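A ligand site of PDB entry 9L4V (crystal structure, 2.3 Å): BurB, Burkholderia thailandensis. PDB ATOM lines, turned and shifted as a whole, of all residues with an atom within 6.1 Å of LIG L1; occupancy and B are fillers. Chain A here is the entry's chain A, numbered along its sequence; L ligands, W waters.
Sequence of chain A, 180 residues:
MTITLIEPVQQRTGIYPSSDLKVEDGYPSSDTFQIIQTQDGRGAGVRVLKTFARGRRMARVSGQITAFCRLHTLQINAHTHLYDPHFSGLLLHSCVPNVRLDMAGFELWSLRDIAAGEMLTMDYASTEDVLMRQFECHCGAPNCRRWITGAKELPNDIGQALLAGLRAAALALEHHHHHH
The backbone carbonyl oxygen (O) of Arg 70 lies within hydrogen-bond range of a nitrogen (N1) of LIG L1 (2.8 Å). The backbone NH (N) of Met 132 sits at hydrogen-bond distance from an oxygen (O2) of LIG L1. The backbone carbonyl oxygen (O) of Thr 73 lies within hydrogen-bond range of a nitrogen (N1) of LIG L1. OE1 of Glu 128 is in salt-bridge range of N1 of LIG L1, 3.999 Å away. The guanidinium group of Arg 133 is in hydrogen-bond range of an oxygen (O4) of LG2 L2 (2.8 Å).
Water W1 lies within hydrogen-bond range of O1 of LIG L1 (2.5 Å), O4 of LG2 L2 (2.7 Å) and O of Arg 133 (2.9 Å). Water W2 lies within hydrogen-bond range of the side-chain carboxylate (OE1) of Glu 128 (2.5 Å), the backbone carbonyl oxygen (O) of Val 130 (2.7 Å), a nitrogen (N1) of LIG L1 (2.8 Å) and the side-chain sulfur (SG) of Cys 69 (3.3 Å).
Merely in contact with LIG L1: Leu 71, Tyr 124, Gly 89, Leu 91, Ser 88, Leu 131, Leu 74, Met 122 and Cys 69. Hydrophobic or aromatic side chains that line LIG L1: Leu 74, Met 122, Tyr 124, Leu 131 and Met 132. Within 4 Å of LIG L1: Cys 69, Arg 70, Leu 71, Thr 73, Leu 74, Ser 88, Gly 89, Leu 91, Met 122, Tyr 124, Glu 128, Leu 131 and Met 132.
The backbone NH (N) of Arg 70 lies within hydrogen-bond range of the side-chain hydroxyl (OG1) of Thr 73 (2.9 Å). The side-chain hydroxyl of Tyr 124 is in hydrogen-bond range of the backbone carbonyl oxygen of Leu 91, at 2.6 Å. The backbone carbonyl oxygen of Gly 89 sits at hydrogen-bond distance from a ring nitrogen (ND1) of His 72, at 3.4 Å. The side-chain carboxylate (OE2) of Glu 128 is in hydrogen-bond range of the side-chain hydroxyl (OG1) of Thr 127, 2.6 Å away. O of Leu 92 sits at hydrogen-bond distance from N of Met 122 (3.1 Å). SG of Cys 69 sits at hydrogen-bond distance from O of Val 130, 3.8 Å away.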
ATOM      1  N   CYS A  69      -4.763  -3.296  -2.513  1.00  0.00           N
ATOM      2  CA  CYS A  69      -5.328  -3.706  -1.244  1.00  0.00           C
ATOM      3  C   CYS A  69      -5.126  -2.598  -0.229  1.00  0.00           C
ATOM      4  O   CYS A  69      -4.047  -2.014  -0.147  1.00  0.00           O
ATOM      5  CB  CYS A  69      -4.684  -5.009  -0.778  1.00  0.00           C
ATOM      6  SG  CYS A  69      -5.486  -5.718   0.714  1.00  0.00           S
ATOM      7  N   ARG A  70      -6.196  -2.279   0.509  1.00  0.00           N
ATOM      8  CA  ARG A  70      -6.202  -1.254   1.552  1.00  0.00           C
ATOM      9  C   ARG A  70      -7.013  -1.772   2.743  1.00  0.00           C
ATOM     10  O   ARG A  70      -7.687  -2.795   2.663  1.00  0.00           O
ATOM     11  CB  ARG A  70      -6.797   0.080   1.068  1.00  0.00           C
ATOM     12  CG  ARG A  70      -6.186   0.668  -0.185  1.00  0.00           C
ATOM     13  CD  ARG A  70      -7.041   1.850  -0.677  1.00  0.00           C
ATOM     14  NE  ARG A  70      -6.889   2.970   0.243  1.00  0.00           N
ATOM     15  CZ  ARG A  70      -7.473   4.153   0.103  1.00  0.00           C
ATOM     16  NH1 ARG A  70      -8.227   4.427  -0.937  1.00  0.00           N
ATOM     17  NH2 ARG A  70      -7.289   5.079   1.051  1.00  0.00           N
ATOM     18  N   LEU A  71      -6.936  -1.053   3.860  1.00  0.00           N
ATOM     19  CA  LEU A  71      -7.630  -1.518   5.058  1.00  0.00           C
ATOM     20  C   LEU A  71      -9.138  -1.642   4.822  1.00  0.00           C
ATOM     21  O   LEU A  71      -9.782  -2.582   5.294  1.00  0.00           O
ATOM     22  CB  LEU A  71      -7.323  -0.609   6.254  1.00  0.00           C
ATOM     23  CG  LEU A  71      -7.969  -1.006   7.593  1.00  0.00           C
ATOM     24  CD1 LEU A  71      -7.413  -2.321   8.141  1.00  0.00           C
ATOM     25  CD2 LEU A  71      -7.885   0.115   8.663  1.00  0.00           C
ATOM     26  N   HIS A  72      -9.714  -0.738   4.021  1.00  0.00           N
ATOM     27  CA  HIS A  72     -11.145  -0.726   3.739  1.00  0.00           C
ATOM     28  C   HIS A  72     -11.488  -1.211   2.332  1.00  0.00           C
ATOM     29  O   HIS A  72     -12.560  -0.878   1.804  1.00  0.00           O
ATOM     30  CB  HIS A  72     -11.710   0.685   3.974  1.00  0.00           C
ATOM     31  CG  HIS A  72     -11.601   1.149   5.404  1.00  0.00           C
ATOM     32  ND1 HIS A  72     -11.912   0.343   6.474  1.00  0.00           N
ATOM     33  CD2 HIS A  72     -11.193   2.328   5.926  1.00  0.00           C
ATOM     34  CE1 HIS A  72     -11.732   1.016   7.607  1.00  0.00           C
ATOM     35  NE2 HIS A  72     -11.298   2.233   7.293  1.00  0.00           N
ATOM     36  N   THR A  73     -10.627  -2.010   1.692  1.00  0.00           N
ATOM     37  CA  THR A  73     -11.007  -2.650   0.444  1.00  0.00           C
ATOM     38  C   THR A  73     -11.478  -4.082   0.690  1.00  0.00           C
ATOM     39  O   THR A  73     -11.138  -4.715   1.696  1.00  0.00           O
ATOM     40  CB  THR A  73      -9.870  -2.707  -0.596  1.00  0.00           C
ATOM     41  OG1 THR A  73      -8.783  -3.492  -0.088  1.00  0.00           O
ATOM     42  CG2 THR A  73      -9.407  -1.324  -1.004  1.00  0.00           C
ATOM     43  N   LEU A  74     -12.234  -4.591  -0.282  1.00  0.00           N
ATOM     44  CA  LEU A  74     -12.504  -6.009  -0.369  1.00  0.00           C
ATOM     45  C   LEU A  74     -12.014  -6.527  -1.716  1.00  0.00           C
ATOM     46  O   LEU A  74     -11.988  -5.804  -2.712  1.00  0.00           O
ATOM     47  CB  LEU A  74     -14.002  -6.315  -0.156  1.00  0.00           C
ATOM     48  CG  LEU A  74     -14.205  -6.139   1.357  1.00  0.00           C
ATOM     49  CD1 LEU A  74     -14.987  -4.891   1.742  1.00  0.00           C
ATOM     50  CD2 LEU A  74     -14.642  -7.386   2.060  1.00  0.00           C
ATOM     51  N   SER A  88     -19.090  -1.941   3.368  1.00  0.00           N
ATOM     52  CA  SER A  88     -18.534  -3.290   3.423  1.00  0.00           C
ATOM     53  C   SER A  88     -17.114  -3.334   3.988  1.00  0.00           C
ATOM     54  O   SER A  88     -16.735  -4.318   4.630  1.00  0.00           O
ATOM     55  CB  SER A  88     -18.593  -3.958   2.030  1.00  0.00           C
ATOM     56  OG  SER A  88     -17.700  -3.354   1.114  1.00  0.00           O
ATOM     57  N   GLY A  89     -16.307  -2.285   3.775  1.00  0.00           N
ATOM     58  CA  GLY A  89     -15.007  -2.222   4.434  1.00  0.00           C
ATOM     59  C   GLY A  89     -15.069  -2.030   5.944  1.00  0.00           C
ATOM     60  O   GLY A  89     -14.067  -2.243   6.648  1.00  0.00           O
ATOM     61  N   LEU A  90     -16.230  -1.652   6.481  1.00  0.00           N
ATOM     62  CA  LEU A  90     -16.380  -1.532   7.919  1.00  0.00           C
ATOM     63  C   LEU A  90     -17.019  -2.774   8.531  1.00  0.00           C
ATOM     64  O   LEU A  90     -17.353  -2.758   9.720  1.00  0.00           O
ATOM     65  CB  LEU A  90     -17.188  -0.286   8.269  1.00  0.00           C
ATOM     66  CG  LEU A  90     -16.666   0.993   7.594  1.00  0.00           C
ATOM     67  CD1 LEU A  90     -17.533   2.197   7.957  1.00  0.00           C
ATOM     68  CD2 LEU A  90     -15.192   1.234   7.956  1.00  0.00           C
ATOM     69  N   LEU A  91     -17.192  -3.845   7.760  1.00  0.00           N
ATOM     70  CA  LEU A  91     -17.644  -5.110   8.342  1.00  0.00           C
ATOM     71  C   LEU A  91     -16.523  -5.737   9.143  1.00  0.00           C
ATOM     72  O   LEU A  91     -15.402  -5.888   8.639  1.00  0.00           O
ATOM     73  CB  LEU A  91     -18.091  -6.076   7.252  1.00  0.00           C
ATOM     74  CG  LEU A  91     -19.340  -5.695   6.490  1.00  0.00           C
ATOM     75  CD1 LEU A  91     -19.450  -6.602   5.251  1.00  0.00           C
ATOM     76  CD2 LEU A  91     -20.569  -5.840   7.397  1.00  0.00           C
ATOM     77  N   LEU A  92     -16.816  -6.112  10.396  1.00  0.00           N
ATOM     78  CA  LEU A  92     -15.807  -6.699  11.271  1.00  0.00           C
ATOM     79  C   LEU A  92     -15.652  -8.169  10.947  1.00  0.00           C
ATOM     80  O   LEU A  92     -16.500  -8.784  10.302  1.00  0.00           O
ATOM     81  CB  LEU A  92     -16.204  -6.551  12.736  1.00  0.00           C
ATOM     82  CG  LEU A  92     -16.396  -5.109  13.215  1.00  0.00           C
ATOM     83  CD1 LEU A  92     -16.979  -5.102  14.630  1.00  0.00           C
ATOM     84  CD2 LEU A  92     -15.059  -4.333  13.128  1.00  0.00           C
ATOM     85  N   LEU A 101     -20.336 -11.884   2.426  1.00  0.00           N
ATOM     86  CA  LEU A 101     -20.218 -10.861   1.404  1.00  0.00           C
ATOM     87  C   LEU A 101     -19.900 -11.539   0.076  1.00  0.00           C
ATOM     88  O   LEU A 101     -18.797 -12.074  -0.126  1.00  0.00           O
ATOM     89  CB  LEU A 101     -19.133  -9.857   1.770  1.00  0.00           C
ATOM     90  CG  LEU A 101     -18.866  -8.771   0.729  1.00  0.00           C
ATOM     91  CD1 LEU A 101     -20.139  -8.002   0.355  1.00  0.00           C
ATOM     92  CD2 LEU A 101     -17.893  -7.832   1.316  1.00  0.00           C
ATOM     93  N   MET A 122     -18.174 -10.996   8.832  1.00  0.00           N
ATOM     94  CA  MET A 122     -17.799 -11.939   7.786  1.00  0.00           C
ATOM     95  C   MET A 122     -16.486 -12.605   8.184  1.00  0.00           C
ATOM     96  O   MET A 122     -15.712 -12.066   8.989  1.00  0.00           O
ATOM     97  CB  MET A 122     -17.534 -11.283   6.426  1.00  0.00           C
ATOM     98  CG  MET A 122     -16.707 -10.028   6.518  1.00  0.00           C
ATOM     99  SD  MET A 122     -16.720  -8.998   5.065  1.00  0.00           S
ATOM    100  CE  MET A 122     -15.954 -10.165   3.926  1.00  0.00           C
ATOM    101  N   TYR A 124     -13.081 -12.791   7.094  1.00  0.00           N
ATOM    102  CA  TYR A 124     -12.202 -12.085   6.145  1.00  0.00           C
ATOM    103  C   TYR A 124     -11.486 -13.057   5.218  1.00  0.00           C
ATOM    104  O   TYR A 124     -11.202 -12.722   4.066  1.00  0.00           O
ATOM    105  CB  TYR A 124     -11.159 -11.247   6.887  1.00  0.00           C
ATOM    106  CG  TYR A 124     -11.662  -9.957   7.521  1.00  0.00           C
ATOM    107  CD1 TYR A 124     -13.009  -9.621   7.524  1.00  0.00           C
ATOM    108  CD2 TYR A 124     -10.769  -9.090   8.143  1.00  0.00           C
ATOM    109  CE1 TYR A 124     -13.459  -8.452   8.127  1.00  0.00           C
ATOM    110  CE2 TYR A 124     -11.207  -7.917   8.737  1.00  0.00           C
ATOM    111  CZ  TYR A 124     -12.543  -7.599   8.735  1.00  0.00           C
ATOM    112  OH  TYR A 124     -12.950  -6.419   9.315  1.00  0.00           O
ATOM    113  N   THR A 127     -13.062 -14.024   1.489  1.00  0.00           N
ATOM    114  CA  THR A 127     -12.897 -13.214   0.281  1.00  0.00           C
ATOM    115  C   THR A 127     -11.457 -12.745   0.027  1.00  0.00           C
ATOM    116  O   THR A 127     -11.133 -12.407  -1.119  1.00  0.00           O
ATOM    117  CB  THR A 127     -13.801 -11.964   0.329  1.00  0.00           C
ATOM    118  OG1 THR A 127     -13.447 -11.165   1.455  1.00  0.00           O
ATOM    119  CG2 THR A 127     -15.311 -12.323   0.431  1.00  0.00           C
ATOM    120  N   GLU A 128     -10.598 -12.725   1.029  1.00  0.00           N
ATOM    121  CA  GLU A 128      -9.293 -12.056   0.938  1.00  0.00           C
ATOM    122  C   GLU A 128      -8.160 -13.076   0.866  1.00  0.00           C
ATOM    123  O   GLU A 128      -8.067 -13.954   1.722  1.00  0.00           O
ATOM    124  CB  GLU A 128      -9.099 -11.129   2.139  1.00  0.00           C
ATOM    125  CG  GLU A 128     -10.289 -10.204   2.408  1.00  0.00           C
ATOM    126  CD  GLU A 128     -10.570  -9.287   1.241  1.00  0.00           C
ATOM    127  OE1 GLU A 128      -9.667  -8.490   0.888  1.00  0.00           O
ATOM    128  OE2 GLU A 128     -11.677  -9.362   0.660  1.00  0.00           O
ATOM    129  N   VAL A 130      -4.942 -11.899   1.103  1.00  0.00           N
ATOM    130  CA  VAL A 130      -4.008 -11.277   2.043  1.00  0.00           C
ATOM    131  C   VAL A 130      -4.682 -10.030   2.616  1.00  0.00           C
ATOM    132  O   VAL A 130      -5.397  -9.312   1.903  1.00  0.00           O
ATOM    133  CB  VAL A 130      -2.659 -10.932   1.355  1.00  0.00           C
ATOM    134  CG1 VAL A 130      -1.656 -10.391   2.349  1.00  0.00           C
ATOM    135  CG2 VAL A 130      -2.036 -12.182   0.702  1.00  0.00           C
ATOM    136  N   LEU A 131      -4.500  -9.791   3.912  1.00  0.00           N
ATOM    137  CA  LEU A 131      -5.035  -8.583   4.529  1.00  0.00           C
ATOM    138  C   LEU A 131      -4.033  -7.435   4.407  1.00  0.00           C
ATOM    139  O   LEU A 131      -2.847  -7.640   4.145  1.00  0.00           O
ATOM    140  CB  LEU A 131      -5.383  -8.828   5.995  1.00  0.00           C
ATOM    141  CG  LEU A 131      -6.433  -9.946   6.248  1.00  0.00           C
ATOM    142  CD1 LEU A 131      -6.723 -10.177   7.724  1.00  0.00           C
ATOM    143  CD2 LEU A 131      -7.747  -9.658   5.494  1.00  0.00           C
ATOM    144  N   MET A 132      -4.544  -6.214   4.558  1.00  0.00           N
ATOM    145  CA  MET A 132      -3.681  -5.057   4.750  1.00  0.00           C
ATOM    146  C   MET A 132      -2.886  -5.177   6.029  1.00  0.00           C
ATOM    147  O   MET A 132      -1.737  -4.709   6.103  1.00  0.00           O
ATOM    148  CB  MET A 132      -4.525  -3.787   4.789  1.00  0.00           C
ATOM    149  CG  MET A 132      -4.275  -2.874   3.652  1.00  0.00           C
ATOM    150  SD  MET A 132      -2.686  -2.072   3.639  1.00  0.00           S
ATOM    151  CE  MET A 132      -2.712  -1.439   5.338  1.00  0.00           C
ATOM    152  N   ARG A 133      -3.480  -5.772   7.061  1.00  0.00           N
ATOM    153  CA  ARG A 133      -2.784  -5.998   8.308  1.00  0.00           C
ATOM    154  C   ARG A 133      -3.416  -7.189   8.999  1.00  0.00           C
ATOM    155  O   ARG A 133      -4.639  -7.416   8.896  1.00  0.00           O
ATOM    156  CB  ARG A 133      -2.821  -4.749   9.217  1.00  0.00           C
ATOM    157  CG  ARG A 133      -4.207  -4.469   9.828  1.00  0.00           C
ATOM    158  CD  ARG A 133      -4.409  -2.984  10.194  1.00  0.00           C
ATOM    159  NE  ARG A 133      -5.575  -2.797  11.061  1.00  0.00           N
ATOM    160  CZ  ARG A 133      -5.981  -1.632  11.551  1.00  0.00           C
ATOM    161  NH1 ARG A 133      -5.299  -0.522  11.334  1.00  0.00           N
ATOM    162  NH2 ARG A 133      -7.100  -1.574  12.268  1.00  0.00           N
ATOM    163  N   PHE A 135      -4.189  -9.220  12.665  1.00  0.00           N
ATOM    164  CA  PHE A 135      -4.621  -8.735  13.965  1.00  0.00           C
ATOM    165  C   PHE A 135      -5.074  -9.894  14.830  1.00  0.00           C
ATOM    166  O   PHE A 135      -5.514 -10.936  14.326  1.00  0.00           O
ATOM    167  CB  PHE A 135      -5.768  -7.727  13.823  1.00  0.00           C
ATOM    168  CG  PHE A 135      -6.974  -8.259  13.084  1.00  0.00           C
ATOM    169  CD1 PHE A 135      -7.999  -8.893  13.768  1.00  0.00           C
ATOM    170  CD2 PHE A 135      -7.084  -8.099  11.705  1.00  0.00           C
ATOM    171  CE1 PHE A 135      -9.134  -9.368  13.074  1.00  0.00           C
ATOM    172  CE2 PHE A 135      -8.190  -8.572  11.015  1.00  0.00           C
ATOM    173  CZ  PHE A 135      -9.225  -9.197  11.701  1.00  0.00           C
HETATM  174  C1  LIG L   1     -12.138  -4.890   6.561  1.00  0.00           C
HETATM  175  S1  LIG L   1     -12.607  -5.556   4.971  1.00  0.00           S
HETATM  176  C2  LIG L   1     -14.120  -6.343   5.605  1.00  0.00           C
HETATM  177  C3  LIG L   1     -11.442  -6.928   5.184  1.00  0.00           C
HETATM  178  C4  LIG L   1     -10.272  -6.828   4.195  1.00  0.00           C
HETATM  179  C5  LIG L   1      -9.370  -5.593   4.351  1.00  0.00           C
HETATM  180  N1  LIG L   1      -8.577  -5.378   3.150  1.00  0.00           N
HETATM  181  C6  LIG L   1      -8.438  -5.764   5.533  1.00  0.00           C
HETATM  182  O1  LIG L   1      -8.914  -5.966   6.769  1.00  0.00           O
HETATM  183  O2  LIG L   1      -7.239  -5.721   5.358  1.00  0.00           O
HETATM  184  N1  LG2 L   2     -12.641  -1.538  12.654  1.00  0.00           N
HETATM  185  C1  LG2 L   2     -12.360  -0.932  11.364  1.00  0.00           C
HETATM  186  C2  LG2 L   2     -12.392   0.514  11.599  1.00  0.00           C
HETATM  187  O1  LG2 L   2     -12.543   0.740  12.817  1.00  0.00           O
HETATM  188  O2  LG2 L   2     -12.251   1.333  10.674  1.00  0.00           O
HETATM  189  C3  LG2 L   2     -13.300  -1.451  10.246  1.00  0.00           C
HETATM  190  C4  LG2 L   2     -13.021  -2.808   9.580  1.00  0.00           C
HETATM  191  S1  LG2 L   2     -11.387  -2.751   9.304  1.00  0.00           S
HETATM  192  C5  LG2 L   2     -11.101  -2.125   7.874  1.00  0.00           C
HETATM  193  C6  LG2 L   2     -10.511  -4.140   9.578  1.00  0.00           C
HETATM  194  C7  LG2 L   2      -9.827  -3.995  10.948  1.00  0.00           C
HETATM  195  O3  LG2 L   2     -10.798  -4.018  12.000  1.00  0.00           O
HETATM  196  C8  LG2 L   2      -8.821  -5.055  11.291  1.00  0.00           C
HETATM  197  O4  LG2 L   2      -7.556  -4.748  10.741  1.00  0.00           O
HETATM  198  C9  LG2 L   2      -8.875  -5.002  12.813  1.00  0.00           C
HETATM  199  O5  LG2 L   2      -8.059  -3.985  13.398  1.00  0.00           O
HETATM  200  C10 LG2 L   2     -10.313  -4.644  13.138  1.00  0.00           C
HETATM  201  N2  LG2 L   2     -11.071  -5.866  13.388  1.00  0.00           N
HETATM  202  C11 LG2 L   2     -12.004  -6.358  12.614  1.00  0.00           C
HETATM  203  N3  LG2 L   2     -12.507  -7.468  13.111  1.00  0.00           N
HETATM  204  C12 LG2 L   2     -11.907  -7.712  14.239  1.00  0.00           C
HETATM  205  C13 LG2 L   2     -11.972  -8.747  15.253  1.00  0.00           C
HETATM  206  N4  LG2 L   2     -12.823  -9.730  15.115  1.00  0.00           N
HETATM  207  N5  LG2 L   2     -11.146  -8.667  16.322  1.00  0.00           N
HETATM  208  C14 LG2 L   2     -10.294  -7.656  16.437  1.00  0.00           C
HETATM  209  N6  LG2 L   2     -10.188  -6.670  15.539  1.00  0.00           N
HETATM  210  C15 LG2 L   2     -10.947  -6.649  14.433  1.00  0.00           C
HETATM  211  O   HOH W   1      -7.330  -6.335   8.616  1.00  0.00           O
HETATM  212  O   HOH W   2      -7.596  -7.825   2.171  1.00  0.00           O
